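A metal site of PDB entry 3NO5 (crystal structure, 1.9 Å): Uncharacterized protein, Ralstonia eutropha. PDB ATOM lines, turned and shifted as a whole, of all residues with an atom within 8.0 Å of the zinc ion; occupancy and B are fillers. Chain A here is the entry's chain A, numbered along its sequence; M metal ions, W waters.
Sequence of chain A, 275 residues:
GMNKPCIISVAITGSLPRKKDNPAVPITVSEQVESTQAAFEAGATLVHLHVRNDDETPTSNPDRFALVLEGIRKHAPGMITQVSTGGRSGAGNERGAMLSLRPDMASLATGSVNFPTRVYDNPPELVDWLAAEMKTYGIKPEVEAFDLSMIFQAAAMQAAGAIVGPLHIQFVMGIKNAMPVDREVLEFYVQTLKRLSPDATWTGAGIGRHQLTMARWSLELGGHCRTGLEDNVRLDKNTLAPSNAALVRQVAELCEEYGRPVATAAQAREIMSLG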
ATOM      1  N   ALA A  11     -10.629  -8.326  22.168  1.00  0.00           N
ATOM      2  CA  ALA A  11      -9.731  -7.425  22.884  1.00  0.00           C
ATOM      3  C   ALA A  11      -9.698  -7.873  24.337  1.00  0.00           C
ATOM      4  O   ALA A  11     -10.628  -7.602  25.099  1.00  0.00           O
ATOM      5  CB  ALA A  11     -10.242  -5.996  22.776  1.00  0.00           C
ATOM      6  N   ILE A  12      -8.674  -8.683  24.680  1.00  0.00           N
ATOM      7  CA  ILE A  12      -8.616  -9.413  25.950  1.00  0.00           C
ATOM      8  C   ILE A  12      -8.377  -8.589  27.224  1.00  0.00           C
ATOM      9  O   ILE A  12      -8.906  -8.958  28.277  1.00  0.00           O
ATOM     10  CB  ILE A  12      -7.647 -10.635  25.847  1.00  0.00           C
ATOM     11  CG1 ILE A  12      -6.185 -10.193  25.519  1.00  0.00           C
ATOM     12  CG2 ILE A  12      -8.162 -11.676  24.845  1.00  0.00           C
ATOM     13  CD1 ILE A  12      -5.111 -11.221  25.881  1.00  0.00           C
ATOM     14  N   THR A  13      -7.510  -7.566  27.167  1.00  0.00           N
ATOM     15  CA  THR A  13      -7.074  -6.873  28.392  1.00  0.00           C
ATOM     16  C   THR A  13      -7.286  -5.358  28.379  1.00  0.00           C
ATOM     17  O   THR A  13      -7.842  -4.811  29.341  1.00  0.00           O
ATOM     18  CB  THR A  13      -5.621  -7.263  28.733  1.00  0.00           C
ATOM     19  OG1 THR A  13      -5.526  -8.693  28.842  1.00  0.00           O
ATOM     20  CG2 THR A  13      -5.106  -6.602  30.011  1.00  0.00           C
ATOM     21  N   GLY A  14      -6.731  -4.686  27.387  1.00  0.00           N
ATOM     22  CA  GLY A  14      -6.746  -3.229  27.332  1.00  0.00           C
ATOM     23  C   GLY A  14      -5.747  -2.606  28.288  1.00  0.00           C
ATOM     24  O   GLY A  14      -4.875  -3.305  28.820  1.00  0.00           O
ATOM     25  N   SER A  15      -5.876  -1.294  28.534  1.00  0.00           N
ATOM     26  CA  SER A  15      -4.954  -0.594  29.435  1.00  0.00           C
ATOM     27  C   SER A  15      -5.642  -0.150  30.746  1.00  0.00           C
ATOM     28  O   SER A  15      -4.945   0.133  31.722  1.00  0.00           O
ATOM     29  CB  SER A  15      -4.326   0.603  28.733  1.00  0.00           C
ATOM     30  OG  SER A  15      -5.320   1.513  28.275  1.00  0.00           O
ATOM     31  N   HIS A  48      -6.800  -8.830  19.787  1.00  0.00           N
ATOM     32  CA  HIS A  48      -6.289  -7.485  19.995  1.00  0.00           C
ATOM     33  C   HIS A  48      -5.569  -7.461  21.338  1.00  0.00           C
ATOM     34  O   HIS A  48      -6.199  -7.666  22.385  1.00  0.00           O
ATOM     35  CB  HIS A  48      -7.425  -6.449  19.959  1.00  0.00           C
ATOM     36  CG  HIS A  48      -6.981  -5.061  20.267  1.00  0.00           C
ATOM     37  ND1 HIS A  48      -6.385  -4.264  19.316  1.00  0.00           N
ATOM     38  CD2 HIS A  48      -7.081  -4.371  21.419  1.00  0.00           C
ATOM     39  CE1 HIS A  48      -6.126  -3.115  19.918  1.00  0.00           C
ATOM     40  NE2 HIS A  48      -6.529  -3.132  21.187  1.00  0.00           N
ATOM     41  N   LEU A  49      -4.238  -7.322  21.306  1.00  0.00           N
ATOM     42  CA  LEU A  49      -3.404  -7.520  22.489  1.00  0.00           C
ATOM     43  C   LEU A  49      -2.802  -6.256  23.083  1.00  0.00           C
ATOM     44  O   LEU A  49      -2.004  -5.575  22.431  1.00  0.00           O
ATOM     45  CB  LEU A  49      -2.300  -8.570  22.194  1.00  0.00           C
ATOM     46  CG  LEU A  49      -1.312  -8.869  23.342  1.00  0.00           C
ATOM     47  CD1 LEU A  49      -2.023  -9.540  24.515  1.00  0.00           C
ATOM     48  CD2 LEU A  49      -0.158  -9.739  22.850  1.00  0.00           C
ATOM     49  N   HIS A  50      -3.107  -6.016  24.371  1.00  0.00           N
ATOM     50  CA  HIS A  50      -2.430  -5.061  25.249  1.00  0.00           C
ATOM     51  C   HIS A  50      -1.710  -5.890  26.297  1.00  0.00           C
ATOM     52  O   HIS A  50      -2.253  -6.909  26.731  1.00  0.00           O
ATOM     53  CB  HIS A  50      -3.454  -4.170  25.963  1.00  0.00           C
ATOM     54  CG  HIS A  50      -4.043  -3.080  25.133  1.00  0.00           C
ATOM     55  ND1 HIS A  50      -3.821  -1.747  25.433  1.00  0.00           N
ATOM     56  CD2 HIS A  50      -4.973  -3.157  24.146  1.00  0.00           C
ATOM     57  CE1 HIS A  50      -4.575  -1.055  24.590  1.00  0.00           C
ATOM     58  NE2 HIS A  50      -5.279  -1.861  23.795  1.00  0.00           N
ATOM     59  N   GLN A  82      -2.838  -9.188  16.816  1.00  0.00           N
ATOM     60  CA  GLN A  82      -2.917  -7.746  16.607  1.00  0.00           C
ATOM     61  C   GLN A  82      -2.456  -6.990  17.852  1.00  0.00           C
ATOM     62  O   GLN A  82      -3.183  -6.939  18.842  1.00  0.00           O
ATOM     63  CB  GLN A  82      -4.344  -7.330  16.213  1.00  0.00           C
ATOM     64  CG  GLN A  82      -4.469  -5.850  15.875  1.00  0.00           C
ATOM     65  CD  GLN A  82      -5.889  -5.477  15.573  1.00  0.00           C
ATOM     66  OE1 GLN A  82      -6.592  -4.910  16.406  1.00  0.00           O
ATOM     67  NE2 GLN A  82      -6.364  -5.869  14.396  1.00  0.00           N
ATOM     68  N   VAL A  83      -1.239  -6.426  17.812  1.00  0.00           N
ATOM     69  CA  VAL A  83      -0.705  -5.676  18.958  1.00  0.00           C
ATOM     70  C   VAL A  83      -1.282  -4.271  18.998  1.00  0.00           C
ATOM     71  O   VAL A  83      -1.604  -3.694  17.963  1.00  0.00           O
ATOM     72  CB  VAL A  83       0.855  -5.672  19.013  1.00  0.00           C
ATOM     73  CG1 VAL A  83       1.419  -7.092  19.086  1.00  0.00           C
ATOM     74  CG2 VAL A  83       1.455  -4.910  17.829  1.00  0.00           C
ATOM     75  N   SER A  84      -1.447  -3.732  20.208  1.00  0.00           N
ATOM     76  CA  SER A  84      -1.915  -2.373  20.372  1.00  0.00           C
ATOM     77  C   SER A  84      -0.744  -1.408  20.374  1.00  0.00           C
ATOM     78  O   SER A  84       0.277  -1.679  21.008  1.00  0.00           O
ATOM     79  CB  SER A  84      -2.702  -2.231  21.666  1.00  0.00           C
ATOM     80  OG  SER A  84      -3.002  -0.867  21.931  1.00  0.00           O
ATOM     81  N   THR A  85      -0.894  -0.259  19.691  1.00  0.00           N
ATOM     82  CA  THR A  85       0.131   0.786  19.703  1.00  0.00           C
ATOM     83  C   THR A  85      -0.376   2.002  20.501  1.00  0.00           C
ATOM     84  O   THR A  85       0.139   3.112  20.331  1.00  0.00           O
ATOM     85  CB  THR A  85       0.553   1.155  18.275  1.00  0.00           C
ATOM     86  OG1 THR A  85      -0.569   1.686  17.571  1.00  0.00           O
ATOM     87  CG2 THR A  85       1.148  -0.043  17.512  1.00  0.00           C
ATOM     88  N   GLY A  86      -1.368   1.775  21.359  1.00  0.00           N
ATOM     89  CA  GLY A  86      -1.914   2.817  22.222  1.00  0.00           C
ATOM     90  C   GLY A  86      -0.958   3.216  23.328  1.00  0.00           C
ATOM     91  O   GLY A  86       0.019   2.516  23.594  1.00  0.00           O
ATOM     92  N   SER A 107      -2.744  -2.087  15.783  1.00  0.00           N
ATOM     93  CA  SER A 107      -3.713  -0.992  15.794  1.00  0.00           C
ATOM     94  C   SER A 107      -3.041   0.320  15.412  1.00  0.00           C
ATOM     95  O   SER A 107      -1.876   0.527  15.745  1.00  0.00           O
ATOM     96  CB  SER A 107      -4.366  -0.869  17.159  1.00  0.00           C
ATOM     97  OG  SER A 107      -5.272  -1.940  17.373  1.00  0.00           O
ATOM     98  N   TYR A 120      -6.815  11.574  23.897  1.00  0.00           N
ATOM     99  CA  TYR A 120      -6.072  10.469  23.304  1.00  0.00           C
ATOM    100  C   TYR A 120      -5.192  11.023  22.194  1.00  0.00           C
ATOM    101  O   TYR A 120      -5.634  11.181  21.058  1.00  0.00           O
ATOM    102  CB  TYR A 120      -7.026   9.364  22.788  1.00  0.00           C
ATOM    103  CG  TYR A 120      -6.283   8.145  22.245  1.00  0.00           C
ATOM    104  CD1 TYR A 120      -5.114   7.691  22.844  1.00  0.00           C
ATOM    105  CD2 TYR A 120      -6.800   7.407  21.181  1.00  0.00           C
ATOM    106  CE1 TYR A 120      -4.424   6.595  22.345  1.00  0.00           C
ATOM    107  CE2 TYR A 120      -6.134   6.285  20.689  1.00  0.00           C
ATOM    108  CZ  TYR A 120      -4.945   5.874  21.273  1.00  0.00           C
ATOM    109  OH  TYR A 120      -4.288   4.773  20.805  1.00  0.00           O
ATOM    110  N   GLU A 142      -4.546  -1.986  11.486  1.00  0.00           N
ATOM    111  CA  GLU A 142      -5.975  -1.855  11.695  1.00  0.00           C
ATOM    112  C   GLU A 142      -6.216  -0.440  12.118  1.00  0.00           C
ATOM    113  O   GLU A 142      -5.794  -0.040  13.206  1.00  0.00           O
ATOM    114  CB  GLU A 142      -6.503  -2.840  12.761  1.00  0.00           C
ATOM    115  CG  GLU A 142      -7.990  -2.634  13.040  1.00  0.00           C
ATOM    116  CD  GLU A 142      -8.613  -3.630  13.999  1.00  0.00           C
ATOM    117  OE1 GLU A 142      -8.978  -4.742  13.553  1.00  0.00           O
ATOM    118  OE2 GLU A 142      -8.816  -3.274  15.187  1.00  0.00           O
ATOM    119  N   GLU A 144      -7.801   2.565  13.678  1.00  0.00           N
ATOM    120  CA  GLU A 144      -8.774   2.812  14.734  1.00  0.00           C
ATOM    121  C   GLU A 144      -9.427   4.154  14.487  1.00  0.00           C
ATOM    122  O   GLU A 144      -8.791   5.194  14.659  1.00  0.00           O
ATOM    123  CB  GLU A 144      -8.112   2.753  16.129  1.00  0.00           C
ATOM    124  CG  GLU A 144      -7.361   1.450  16.422  1.00  0.00           C
ATOM    125  CD  GLU A 144      -8.187   0.171  16.337  1.00  0.00           C
ATOM    126  OE1 GLU A 144      -9.415   0.239  16.562  1.00  0.00           O
ATOM    127  OE2 GLU A 144      -7.590  -0.895  16.087  1.00  0.00           O
ATOM    128  N   PHE A 146     -11.807   6.684  15.681  1.00  0.00           N
ATOM    129  CA  PHE A 146     -12.567   7.170  16.842  1.00  0.00           C
ATOM    130  C   PHE A 146     -13.419   8.384  16.451  1.00  0.00           C
ATOM    131  O   PHE A 146     -14.228   8.862  17.256  1.00  0.00           O
ATOM    132  CB  PHE A 146     -11.617   7.540  17.987  1.00  0.00           C
ATOM    133  CG  PHE A 146     -10.879   6.365  18.590  1.00  0.00           C
ATOM    134  CD1 PHE A 146      -9.614   6.008  18.138  1.00  0.00           C
ATOM    135  CD2 PHE A 146     -11.422   5.668  19.663  1.00  0.00           C
ATOM    136  CE1 PHE A 146      -8.921   4.949  18.719  1.00  0.00           C
ATOM    137  CE2 PHE A 146     -10.717   4.601  20.246  1.00  0.00           C
ATOM    138  CZ  PHE A 146      -9.480   4.244  19.763  1.00  0.00           C
ATOM    139  N   GLN A 170     -11.518   0.028  11.950  1.00  0.00           N
ATOM    140  CA  GLN A 170     -12.414  -0.261  13.046  1.00  0.00           C
ATOM    141  C   GLN A 170     -13.133   0.998  13.494  1.00  0.00           C
ATOM    142  O   GLN A 170     -12.479   1.977  13.881  1.00  0.00           O
ATOM    143  CB  GLN A 170     -11.647  -0.905  14.205  1.00  0.00           C
ATOM    144  CG  GLN A 170     -12.533  -1.283  15.370  1.00  0.00           C
ATOM    145  CD  GLN A 170     -11.873  -2.293  16.250  1.00  0.00           C
ATOM    146  OE1 GLN A 170     -12.038  -3.495  16.065  1.00  0.00           O
ATOM    147  NE2 GLN A 170     -11.078  -1.822  17.202  1.00  0.00           N
ATOM    148  N   ARG A 226     -16.243  -7.092  17.113  1.00  0.00           N
ATOM    149  CA  ARG A 226     -15.233  -7.048  18.151  1.00  0.00           C
ATOM    150  C   ARG A 226     -15.895  -7.108  19.525  1.00  0.00           C
ATOM    151  O   ARG A 226     -16.896  -6.435  19.770  1.00  0.00           O
ATOM    152  CB  ARG A 226     -14.359  -5.779  18.029  1.00  0.00           C
ATOM    153  CG  ARG A 226     -13.431  -5.567  19.240  1.00  0.00           C
ATOM    154  CD  ARG A 226     -12.489  -4.395  19.069  1.00  0.00           C
ATOM    155  NE  ARG A 226     -12.139  -3.789  20.354  1.00  0.00           N
ATOM    156  CZ  ARG A 226     -10.953  -3.239  20.623  1.00  0.00           C
ATOM    157  NH1 ARG A 226      -9.976  -3.290  19.724  1.00  0.00           N
ATOM    158  NH2 ARG A 226     -10.720  -2.693  21.808  1.00  0.00           N
ATOM    159  N   GLU A 230     -11.584  -5.730  27.449  1.00  0.00           N
ATOM    160  CA  GLU A 230     -10.974  -4.409  27.210  1.00  0.00           C
ATOM    161  C   GLU A 230     -12.059  -3.333  27.018  1.00  0.00           C
ATOM    162  O   GLU A 230     -11.923  -2.214  27.515  1.00  0.00           O
ATOM    163  CB  GLU A 230     -10.051  -4.469  25.979  1.00  0.00           C
ATOM    164  CG  GLU A 230      -9.695  -3.109  25.386  1.00  0.00           C
ATOM    165  CD  GLU A 230      -8.599  -3.140  24.345  1.00  0.00           C
ATOM    166  OE1 GLU A 230      -7.848  -4.149  24.306  1.00  0.00           O
ATOM    167  OE2 GLU A 230      -8.434  -2.134  23.615  1.00  0.00           O
ATOM    168  N   ASP A 231     -13.142  -3.689  26.296  1.00  0.00           N
ATOM    169  CA  ASP A 231     -14.222  -2.757  25.975  1.00  0.00           C
ATOM    170  C   ASP A 231     -15.377  -2.826  26.965  1.00  0.00           C
ATOM    171  O   ASP A 231     -16.081  -1.837  27.145  1.00  0.00           O
ATOM    172  CB  ASP A 231     -14.733  -3.014  24.558  1.00  0.00           C
ATOM    173  CG  ASP A 231     -13.659  -2.949  23.491  1.00  0.00           C
ATOM    174  OD1 ASP A 231     -12.750  -2.109  23.619  1.00  0.00           O
ATOM    175  OD2 ASP A 231     -13.743  -3.729  22.516  1.00  0.00           O
HETATM  176 ZN    ZN M   1      -6.861  -1.447  22.451  1.00  0.00          ZN
HETATM  177  O   HOH W   1      -7.290   0.349  23.508  1.00  0.00           O
HETATM  178  O   HOH W   2      -5.555  -0.174  21.361  1.00  0.00           O
HETATM  179  O   HOH W   3      -8.361  -0.816  20.896  1.00  0.00           O
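The backbone NH (N) of Gly 14 is in hydrogen-bond range of the side-chain carboxylate (OE1) of Glu 230.
The backbone NH (N) of Glu 230 is in hydrogen-bond range of the backbone carbonyl oxygen (O) of Ala 11 (3.2 Å).
O of Leu 49 sits at hydrogen-bond distance from N of Ser 84.
NH2 of Arg 226 lies close to OE2 of Glu 230, 3.0 Å away.
A ring nitrogen (NE2) of His 50 sits close to the side-chain hydroxyl (OG) of Ser 84.
The backbone NH of Gly 86 is in hydrogen-bond range of the side-chain hydroxyl of Ser 84 (3.2 Å).
A ring nitrogen (ND1) of His 48 lies close to the side-chain hydroxyl of Ser 107 (3.2 Å).
The side-chain amide oxygen of Gln 82 lies within hydrogen-bond range of a ring nitrogen (ND1) of His 48.
Ser 84 touches the zinc ion.
Within 4 Å of the zinc ion: His 48, His 50, Ser 84 and Glu 230.
The zinc ion is bound by OE2 of Glu 230 (2.1 Å), NE2 of His 50 (2.1 Å), water W2 (2.1 Å), water W1 (2.1 Å), NE2 of His 48 (2.1 Å) and water W3 (2.3 Å).
The zinc ion has six donor atoms within binding distance.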
